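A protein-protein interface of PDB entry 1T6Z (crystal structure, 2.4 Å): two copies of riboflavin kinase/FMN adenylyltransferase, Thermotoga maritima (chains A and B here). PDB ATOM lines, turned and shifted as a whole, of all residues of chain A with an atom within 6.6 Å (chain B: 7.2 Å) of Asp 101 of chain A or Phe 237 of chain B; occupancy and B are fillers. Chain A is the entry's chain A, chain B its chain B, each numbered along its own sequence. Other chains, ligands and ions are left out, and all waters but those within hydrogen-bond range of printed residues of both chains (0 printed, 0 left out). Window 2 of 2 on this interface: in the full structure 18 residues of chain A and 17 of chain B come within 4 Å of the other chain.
Among the printed residues, pairs that only touch across the chains: Asp 101 of chain A with Asp 236 of chain B and Asp 101 of chain A with Glu 238 of chain B.
Of the printed residues of chain B, Arg 100 of chain A touches Glu 238 (3.6 Å). Asp 101 of chain A touches just these residues of chain B: Asp 236 (3.5 Å), Phe 237 (3.5 Å) and Glu 238 (3.8 Å). Of the printed residues of chain B, Arg 134 of chain A touches Glu 238 (2.5 Å). Leu 235 of chain B touches none of the printed residues of chain A. Printed residues of chain A within 4 Å of Asp 236 of chain B: Asp 101 (3.5 Å) and Arg 103 (3.1 Å). Of chain A, only Asp 101 comes within 4 Å of Phe 237 of chain B. Of the printed residues of chain A, Glu 238 of chain B touches Arg 100 (3.6 Å), Asp 101 (3.8 Å) and Arg 134 (2.5 Å). Gly 239 of chain B touches none of the printed residues of chain A. The nearest residue of chain B that does not touch Asp 101 of chain A is Lys 210 of chain B (4.7 Å).
OD2 of Asp 101 of chain A is in hydrogen-bond range of N of Phe 237 of chain B (3.5 Å). The guanidinium group of Arg 134 of chain A lies within hydrogen-bond range of the backbone carbonyl oxygen of Glu 238 of chain B. The guanidinium group of Arg 100 of chain A lies within salt-bridge range of the side-chain carboxylate of Glu 238 of chain B (3.6 Å). NH2 of Arg 103 of chain A lies close to NH2 of Arg 278 of chain B. The guanidinium group (NE) of Arg 103 of chain A lies within salt-bridge range of the side-chain carboxylate (OD2) of Asp 236 of chain B, at 3.4 Å.
Of the 19 printed residues of chain B, 4 touch a printed residue of chain A. Printed residues of chain B that touch a printed residue of chain A: Asp 236, Phe 237, Glu 238 and Arg 278. Of the 8 printed residues of chain A, 4 touch a printed residue of chain B. Printed residues of chain A that touch a printed residue of chain B: Arg 100, Asp 101, Arg 103 and Arg 134. Among the printed residues, Asp or Glu carboxylates within 4 Å of a Lys or Arg side-chain nitrogen of the other chain: Arg 100 of chain A with Glu 238 of chain B and Arg 103 of chain A with Asp 236 of chain B.
OE1 of Glu 124 of chain A lies within salt-bridge range of NH1 of Arg 100 of chain A (3.2 Å). The backbone carbonyl oxygen (O) of Asp 236 of chain B lies within hydrogen-bond range of the side-chain amino group (NZ) of Lys 210 of chain B, 2.7 Å away. OD2 of Asp 236 of chain B lies within salt-bridge range of NH2 of Arg 278 of chain B, at 2.6 Å. The guanidinium group (NH2) of Arg 134 of chain A is in salt-bridge range of the side-chain carboxylate (OD1) of Asp 127 of chain A, 3.4 Å away.
No position is printed for both chains.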
ATOM      1  N   GLY A  99      13.775  39.058 -12.236  1.00  0.00           N
ATOM      2  CA  GLY A  99      12.600  38.741 -11.445  1.00  0.00           C
ATOM      3  C   GLY A  99      12.994  37.864 -10.268  1.00  0.00           C
ATOM      4  O   GLY A  99      14.127  37.386 -10.170  1.00  0.00           O
ATOM      5  N   ARG A 100      12.056  37.650  -9.359  1.00  0.00           N
ATOM      6  CA  ARG A 100      12.302  36.812  -8.193  1.00  0.00           C
ATOM      7  C   ARG A 100      12.521  35.354  -8.630  1.00  0.00           C
ATOM      8  O   ARG A 100      12.069  34.932  -9.701  1.00  0.00           O
ATOM      9  CB  ARG A 100      11.105  36.909  -7.251  1.00  0.00           C
ATOM     10  CG  ARG A 100      10.831  38.319  -6.759  1.00  0.00           C
ATOM     11  CD  ARG A 100      11.801  38.680  -5.663  1.00  0.00           C
ATOM     12  NE  ARG A 100      11.637  37.772  -4.535  1.00  0.00           N
ATOM     13  CZ  ARG A 100      12.458  37.713  -3.494  1.00  0.00           C
ATOM     14  NH1 ARG A 100      13.513  38.516  -3.428  1.00  0.00           N
ATOM     15  NH2 ARG A 100      12.220  36.844  -2.521  1.00  0.00           N
ATOM     16  N   ASP A 101      13.216  34.581  -7.807  1.00  0.00           N
ATOM     17  CA  ASP A 101      13.465  33.186  -8.153  1.00  0.00           C
ATOM     18  C   ASP A 101      14.231  33.074  -9.492  1.00  0.00           C
ATOM     19  O   ASP A 101      13.993  32.149 -10.278  1.00  0.00           O
ATOM     20  CB  ASP A 101      12.128  32.430  -8.275  1.00  0.00           C
ATOM     21  CG  ASP A 101      11.272  32.495  -7.002  1.00  0.00           C
ATOM     22  OD1 ASP A 101      10.094  32.908  -7.123  1.00  0.00           O
ATOM     23  OD2 ASP A 101      11.753  32.121  -5.900  1.00  0.00           O
ATOM     24  N   PHE A 102      15.135  34.018  -9.759  1.00  0.00           N
ATOM     25  CA  PHE A 102      15.890  33.975 -10.999  1.00  0.00           C
ATOM     26  C   PHE A 102      16.979  32.928 -10.885  1.00  0.00           C
ATOM     27  O   PHE A 102      17.660  32.838  -9.865  1.00  0.00           O
ATOM     28  CB  PHE A 102      16.517  35.322 -11.337  1.00  0.00           C
ATOM     29  CG  PHE A 102      17.337  35.292 -12.598  1.00  0.00           C
ATOM     30  CD1 PHE A 102      16.720  35.184 -13.841  1.00  0.00           C
ATOM     31  CD2 PHE A 102      18.734  35.314 -12.542  1.00  0.00           C
ATOM     32  CE1 PHE A 102      17.479  35.096 -15.014  1.00  0.00           C
ATOM     33  CE2 PHE A 102      19.501  35.226 -13.710  1.00  0.00           C
ATOM     34  CZ  PHE A 102      18.871  35.117 -14.946  1.00  0.00           C
ATOM     35  N   ARG A 103      17.132  32.142 -11.948  1.00  0.00           N
ATOM     36  CA  ARG A 103      18.113  31.068 -12.000  1.00  0.00           C
ATOM     37  C   ARG A 103      18.813  31.021 -13.350  1.00  0.00           C
ATOM     38  O   ARG A 103      18.282  31.485 -14.365  1.00  0.00           O
ATOM     39  CB  ARG A 103      17.414  29.733 -11.741  1.00  0.00           C
ATOM     40  CG  ARG A 103      16.963  29.541 -10.313  1.00  0.00           C
ATOM     41  CD  ARG A 103      18.094  28.934  -9.503  1.00  0.00           C
ATOM     42  NE  ARG A 103      17.798  28.897  -8.078  1.00  0.00           N
ATOM     43  CZ  ARG A 103      18.520  28.233  -7.177  1.00  0.00           C
ATOM     44  NH1 ARG A 103      19.589  27.533  -7.548  1.00  0.00           N
ATOM     45  NH2 ARG A 103      18.186  28.292  -5.890  1.00  0.00           N
ATOM     46  N   GLU A 124      16.387  42.490  -7.450  1.00  0.00           N
ATOM     47  CA  GLU A 124      15.314  41.535  -7.601  1.00  0.00           C
ATOM     48  C   GLU A 124      13.956  42.232  -7.618  1.00  0.00           C
ATOM     49  O   GLU A 124      13.482  42.699  -6.582  1.00  0.00           O
ATOM     50  CB  GLU A 124      15.379  40.535  -6.467  1.00  0.00           C
ATOM     51  CG  GLU A 124      16.672  39.775  -6.448  1.00  0.00           C
ATOM     52  CD  GLU A 124      16.650  38.635  -5.461  1.00  0.00           C
ATOM     53  OE1 GLU A 124      16.625  38.905  -4.237  1.00  0.00           O
ATOM     54  OE2 GLU A 124      16.651  37.467  -5.916  1.00  0.00           O
ATOM     55  N   ASP A 127       7.075  40.534  -8.363  1.00  0.00           N
ATOM     56  CA  ASP A 127       6.019  40.265  -9.332  1.00  0.00           C
ATOM     57  C   ASP A 127       4.874  41.247  -9.184  1.00  0.00           C
ATOM     58  O   ASP A 127       4.571  41.702  -8.078  1.00  0.00           O
ATOM     59  CB  ASP A 127       5.486  38.846  -9.134  1.00  0.00           C
ATOM     60  CG  ASP A 127       6.174  37.844 -10.023  1.00  0.00           C
ATOM     61  OD1 ASP A 127       6.173  36.641  -9.676  1.00  0.00           O
ATOM     62  OD2 ASP A 127       6.701  38.272 -11.079  1.00  0.00           O
ATOM     63  N   ARG A 134      -0.461  36.861  -9.678  1.00  0.00           N
ATOM     64  CA  ARG A 134       0.859  37.346 -10.072  1.00  0.00           C
ATOM     65  C   ARG A 134       0.967  37.251 -11.586  1.00  0.00           C
ATOM     66  O   ARG A 134       0.836  36.173 -12.151  1.00  0.00           O
ATOM     67  CB  ARG A 134       1.937  36.487  -9.416  1.00  0.00           C
ATOM     68  CG  ARG A 134       1.621  36.157  -7.981  1.00  0.00           C
ATOM     69  CD  ARG A 134       2.693  35.307  -7.356  1.00  0.00           C
ATOM     70  NE  ARG A 134       3.903  36.075  -7.104  1.00  0.00           N
ATOM     71  CZ  ARG A 134       4.981  35.582  -6.502  1.00  0.00           C
ATOM     72  NH1 ARG A 134       4.986  34.316  -6.097  1.00  0.00           N
ATOM     73  NH2 ARG A 134       6.054  36.347  -6.302  1.00  0.00           N
ATOM     74  N   PRO B 179       9.827  26.273   3.390  1.00  0.00           N
ATOM     75  CA  PRO B 179       8.395  26.115   3.087  1.00  0.00           C
ATOM     76  C   PRO B 179       7.939  24.918   2.241  1.00  0.00           C
ATOM     77  O   PRO B 179       8.350  24.770   1.093  1.00  0.00           O
ATOM     78  CB  PRO B 179       8.042  27.442   2.415  1.00  0.00           C
ATOM     79  CG  PRO B 179       8.956  28.408   3.091  1.00  0.00           C
ATOM     80  CD  PRO B 179      10.266  27.649   3.088  1.00  0.00           C
ATOM     81  N   LEU B 204       0.492  24.629 -10.469  1.00  0.00           N
ATOM     82  CA  LEU B 204      -0.108  25.643  -9.612  1.00  0.00           C
ATOM     83  C   LEU B 204      -1.407  26.225 -10.142  1.00  0.00           C
ATOM     84  O   LEU B 204      -1.786  26.004 -11.294  1.00  0.00           O
ATOM     85  CB  LEU B 204       0.898  26.771  -9.357  1.00  0.00           C
ATOM     86  CG  LEU B 204       2.238  26.446  -8.679  1.00  0.00           C
ATOM     87  CD1 LEU B 204       3.010  27.730  -8.509  1.00  0.00           C
ATOM     88  CD2 LEU B 204       2.026  25.804  -7.337  1.00  0.00           C
ATOM     89  N   PRO B 205      -2.114  26.977  -9.286  1.00  0.00           N
ATOM     90  CA  PRO B 205      -3.397  27.631  -9.573  1.00  0.00           C
ATOM     91  C   PRO B 205      -3.418  28.535 -10.808  1.00  0.00           C
ATOM     92  O   PRO B 205      -4.322  28.437 -11.643  1.00  0.00           O
ATOM     93  CB  PRO B 205      -3.675  28.409  -8.287  1.00  0.00           C
ATOM     94  CG  PRO B 205      -3.031  27.534  -7.221  1.00  0.00           C
ATOM     95  CD  PRO B 205      -1.729  27.171  -7.874  1.00  0.00           C
ATOM     96  N   ASP B 206      -2.431  29.422 -10.910  1.00  0.00           N
ATOM     97  CA  ASP B 206      -2.349  30.352 -12.034  1.00  0.00           C
ATOM     98  C   ASP B 206      -2.483  29.583 -13.342  1.00  0.00           C
ATOM     99  O   ASP B 206      -3.485  29.693 -14.053  1.00  0.00           O
ATOM    100  CB  ASP B 206      -1.000  31.089 -12.036  1.00  0.00           C
ATOM    101  CG  ASP B 206      -0.513  31.449 -10.636  1.00  0.00           C
ATOM    102  OD1 ASP B 206      -0.075  30.539  -9.892  1.00  0.00           O
ATOM    103  OD2 ASP B 206      -0.566  32.649 -10.286  1.00  0.00           O
ATOM    104  N   LYS B 208       0.808  28.090 -13.899  1.00  0.00           N
ATOM    105  CA  LYS B 208       2.246  27.947 -13.740  1.00  0.00           C
ATOM    106  C   LYS B 208       2.696  26.546 -13.344  1.00  0.00           C
ATOM    107  O   LYS B 208       2.083  25.910 -12.490  1.00  0.00           O
ATOM    108  CB  LYS B 208       2.699  28.961 -12.688  1.00  0.00           C
ATOM    109  CG  LYS B 208       4.159  28.911 -12.300  1.00  0.00           C
ATOM    110  CD  LYS B 208       4.520  30.083 -11.376  1.00  0.00           C
ATOM    111  CE  LYS B 208       4.636  31.418 -12.129  1.00  0.00           C
ATOM    112  NZ  LYS B 208       5.797  31.446 -13.087  1.00  0.00           N
ATOM    113  N   LYS B 210       5.929  24.289 -11.912  1.00  0.00           N
ATOM    114  CA  LYS B 210       7.205  24.357 -11.215  1.00  0.00           C
ATOM    115  C   LYS B 210       7.537  22.954 -10.720  1.00  0.00           C
ATOM    116  O   LYS B 210       6.632  22.225 -10.312  1.00  0.00           O
ATOM    117  CB  LYS B 210       7.095  25.277  -9.994  1.00  0.00           C
ATOM    118  CG  LYS B 210       6.739  26.734 -10.270  1.00  0.00           C
ATOM    119  CD  LYS B 210       7.979  27.548 -10.584  1.00  0.00           C
ATOM    120  CE  LYS B 210       7.678  29.041 -10.535  1.00  0.00           C
ATOM    121  NZ  LYS B 210       8.900  29.899 -10.666  1.00  0.00           N
ATOM    122  N   PHE B 211       8.814  22.572 -10.745  1.00  0.00           N
ATOM    123  CA  PHE B 211       9.200  21.255 -10.247  1.00  0.00           C
ATOM    124  C   PHE B 211       9.201  21.378  -8.747  1.00  0.00           C
ATOM    125  O   PHE B 211       9.092  22.490  -8.215  1.00  0.00           O
ATOM    126  CB  PHE B 211      10.574  20.835 -10.758  1.00  0.00           C
ATOM    127  CG  PHE B 211      10.553  20.296 -12.167  1.00  0.00           C
ATOM    128  CD1 PHE B 211      10.636  18.920 -12.408  1.00  0.00           C
ATOM    129  CD2 PHE B 211      10.438  21.152 -13.254  1.00  0.00           C
ATOM    130  CE1 PHE B 211      10.606  18.406 -13.726  1.00  0.00           C
ATOM    131  CE2 PHE B 211      10.405  20.653 -14.574  1.00  0.00           C
ATOM    132  CZ  PHE B 211      10.491  19.284 -14.807  1.00  0.00           C
ATOM    133  N   TYR B 233       8.040  20.385  -1.480  1.00  0.00           N
ATOM    134  CA  TYR B 233       8.934  21.533  -1.430  1.00  0.00           C
ATOM    135  C   TYR B 233       9.027  22.056  -2.854  1.00  0.00           C
ATOM    136  O   TYR B 233       9.723  21.471  -3.690  1.00  0.00           O
ATOM    137  CB  TYR B 233      10.334  21.113  -0.946  1.00  0.00           C
ATOM    138  CG  TYR B 233      11.365  22.214  -1.080  1.00  0.00           C
ATOM    139  CD1 TYR B 233      11.315  23.348  -0.272  1.00  0.00           C
ATOM    140  CD2 TYR B 233      12.325  22.169  -2.083  1.00  0.00           C
ATOM    141  CE1 TYR B 233      12.189  24.414  -0.467  1.00  0.00           C
ATOM    142  CE2 TYR B 233      13.200  23.229  -2.288  1.00  0.00           C
ATOM    143  CZ  TYR B 233      13.124  24.349  -1.479  1.00  0.00           C
ATOM    144  OH  TYR B 233      13.971  25.410  -1.706  1.00  0.00           O
ATOM    145  N   ILE B 234       8.334  23.150  -3.140  1.00  0.00           N
ATOM    146  CA  ILE B 234       8.360  23.693  -4.490  1.00  0.00           C
ATOM    147  C   ILE B 234       9.625  24.500  -4.756  1.00  0.00           C
ATOM    148  O   ILE B 234       9.971  25.405  -3.991  1.00  0.00           O
ATOM    149  CB  ILE B 234       7.141  24.574  -4.750  1.00  0.00           C
ATOM    150  CG1 ILE B 234       5.880  23.879  -4.208  1.00  0.00           C
ATOM    151  CG2 ILE B 234       7.010  24.838  -6.240  1.00  0.00           C
ATOM    152  CD1 ILE B 234       4.574  24.681  -4.370  1.00  0.00           C
ATOM    153  N   LEU B 235      10.315  24.153  -5.841  1.00  0.00           N
ATOM    154  CA  LEU B 235      11.550  24.830  -6.244  1.00  0.00           C
ATOM    155  C   LEU B 235      11.311  26.155  -6.949  1.00  0.00           C
ATOM    156  O   LEU B 235      10.352  26.314  -7.695  1.00  0.00           O
ATOM    157  CB  LEU B 235      12.378  23.948  -7.183  1.00  0.00           C
ATOM    158  CG  LEU B 235      13.217  22.826  -6.591  1.00  0.00           C
ATOM    159  CD1 LEU B 235      12.320  21.735  -6.064  1.00  0.00           C
ATOM    160  CD2 LEU B 235      14.131  22.289  -7.662  1.00  0.00           C
ATOM    161  N   ASP B 236      12.213  27.097  -6.710  1.00  0.00           N
ATOM    162  CA  ASP B 236      12.156  28.414  -7.329  1.00  0.00           C
ATOM    163  C   ASP B 236      10.751  29.011  -7.320  1.00  0.00           C
ATOM    164  O   ASP B 236      10.228  29.451  -8.352  1.00  0.00           O
ATOM    165  CB  ASP B 236      12.674  28.329  -8.764  1.00  0.00           C
ATOM    166  CG  ASP B 236      14.088  27.769  -8.852  1.00  0.00           C
ATOM    167  OD1 ASP B 236      14.547  27.552 -10.000  1.00  0.00           O
ATOM    168  OD2 ASP B 236      14.735  27.547  -7.797  1.00  0.00           O
ATOM    169  N   PHE B 237      10.158  29.046  -6.136  1.00  0.00           N
ATOM    170  CA  PHE B 237       8.807  29.567  -5.967  1.00  0.00           C
ATOM    171  C   PHE B 237       8.621  30.152  -4.568  1.00  0.00           C
ATOM    172  O   PHE B 237       9.161  29.629  -3.587  1.00  0.00           O
ATOM    173  CB  PHE B 237       7.795  28.429  -6.178  1.00  0.00           C
ATOM    174  CG  PHE B 237       6.400  28.761  -5.727  1.00  0.00           C
ATOM    175  CD1 PHE B 237       5.499  29.372  -6.595  1.00  0.00           C
ATOM    176  CD2 PHE B 237       5.995  28.482  -4.421  1.00  0.00           C
ATOM    177  CE1 PHE B 237       4.206  29.701  -6.167  1.00  0.00           C
ATOM    178  CE2 PHE B 237       4.716  28.803  -3.982  1.00  0.00           C
ATOM    179  CZ  PHE B 237       3.815  29.414  -4.857  1.00  0.00           C
ATOM    180  N   GLU B 238       7.868  31.241  -4.476  1.00  0.00           N
ATOM    181  CA  GLU B 238       7.588  31.831  -3.168  1.00  0.00           C
ATOM    182  C   GLU B 238       6.198  32.428  -3.104  1.00  0.00           C
ATOM    183  O   GLU B 238       5.771  33.130  -4.015  1.00  0.00           O
ATOM    184  CB  GLU B 238       8.640  32.872  -2.787  1.00  0.00           C
ATOM    185  CG  GLU B 238       9.890  32.246  -2.177  1.00  0.00           C
ATOM    186  CD  GLU B 238      10.286  32.879  -0.857  1.00  0.00           C
ATOM    187  OE1 GLU B 238      10.596  34.092  -0.842  1.00  0.00           O
ATOM    188  OE2 GLU B 238      10.289  32.158   0.165  1.00  0.00           O
ATOM    189  N   GLY B 239       5.485  32.113  -2.026  1.00  0.00           N
ATOM    190  CA  GLY B 239       4.134  32.612  -1.836  1.00  0.00           C
ATOM    191  C   GLY B 239       3.325  31.629  -1.016  1.00  0.00           C
ATOM    192  O   GLY B 239       3.809  30.540  -0.703  1.00  0.00           O
ATOM    193  N   ASP B 240       2.099  31.997  -0.653  1.00  0.00           N
ATOM    194  CA  ASP B 240       1.272  31.085   0.125  1.00  0.00           C
ATOM    195  C   ASP B 240       0.182  30.471  -0.745  1.00  0.00           C
ATOM    196  O   ASP B 240      -0.378  31.116  -1.635  1.00  0.00           O
ATOM    197  CB  ASP B 240       0.664  31.785   1.353  1.00  0.00           C
ATOM    198  CG  ASP B 240      -0.381  32.818   0.987  1.00  0.00           C
ATOM    199  OD1 ASP B 240      -0.032  33.796   0.294  1.00  0.00           O
ATOM    200  OD2 ASP B 240      -1.550  32.650   1.399  1.00  0.00           O
ATOM    201  N   LEU B 241      -0.105  29.206  -0.470  1.00  0.00           N
ATOM    202  CA  LEU B 241      -1.087  28.456  -1.225  1.00  0.00           C
ATOM    203  C   LEU B 241      -2.171  27.852  -0.353  1.00  0.00           C
ATOM    204  O   LEU B 241      -2.874  26.934  -0.791  1.00  0.00           O
ATOM    205  CB  LEU B 241      -0.369  27.351  -1.979  1.00  0.00           C
ATOM    206  CG  LEU B 241       0.653  27.912  -2.951  1.00  0.00           C
ATOM    207  CD1 LEU B 241       1.701  26.876  -3.290  1.00  0.00           C
ATOM    208  CD2 LEU B 241      -0.081  28.390  -4.173  1.00  0.00           C
ATOM    209  N   GLN B 244      -5.592  26.655  -1.715  1.00  0.00           N
ATOM    210  CA  GLN B 244      -5.549  26.472  -3.164  1.00  0.00           C
ATOM    211  C   GLN B 244      -5.223  25.044  -3.571  1.00  0.00           C
ATOM    212  O   GLN B 244      -4.574  24.316  -2.822  1.00  0.00           O
ATOM    213  CB  GLN B 244      -4.531  27.429  -3.776  1.00  0.00           C
ATOM    214  CG  GLN B 244      -4.954  28.882  -3.704  1.00  0.00           C
ATOM    215  CD  GLN B 244      -4.197  29.747  -4.692  1.00  0.00           C
ATOM    216  OE1 GLN B 244      -3.096  30.228  -4.404  1.00  0.00           O
ATOM    217  NE2 GLN B 244      -4.778  29.933  -5.881  1.00  0.00           N
ATOM    218  N   LEU B 246      -3.450  21.947  -5.834  1.00  0.00           N
ATOM    219  CA  LEU B 246      -2.180  21.628  -6.476  1.00  0.00           C
ATOM    220  C   LEU B 246      -2.289  20.257  -7.112  1.00  0.00           C
ATOM    221  O   LEU B 246      -2.831  19.330  -6.507  1.00  0.00           O
ATOM    222  CB  LEU B 246      -1.030  21.584  -5.467  1.00  0.00           C
ATOM    223  CG  LEU B 246      -0.466  22.877  -4.884  1.00  0.00           C
ATOM    224  CD1 LEU B 246       0.798  22.565  -4.112  1.00  0.00           C
ATOM    225  CD2 LEU B 246      -0.160  23.843  -6.007  1.00  0.00           C
ATOM    226  N   ARG B 278      17.486  19.050  -8.932  1.00  0.00           N
ATOM    227  CA  ARG B 278      17.977  19.949  -9.977  1.00  0.00           C
ATOM    228  C   ARG B 278      18.825  19.273 -11.063  1.00  0.00           C
ATOM    229  O   ARG B 278      18.815  19.719 -12.211  1.00  0.00           O
ATOM    230  CB  ARG B 278      18.735  21.118  -9.341  1.00  0.00           C
ATOM    231  CG  ARG B 278      17.855  22.030  -8.488  1.00  0.00           C
ATOM    232  CD  ARG B 278      18.582  23.312  -8.053  1.00  0.00           C
ATOM    233  NE  ARG B 278      17.793  24.144  -7.137  1.00  0.00           N
ATOM    234  CZ  ARG B 278      16.937  25.095  -7.511  1.00  0.00           C
ATOM    235  NH1 ARG B 278      16.737  25.360  -8.795  1.00  0.00           N
ATOM    236  NH2 ARG B 278      16.280  25.797  -6.594  1.00  0.00           N
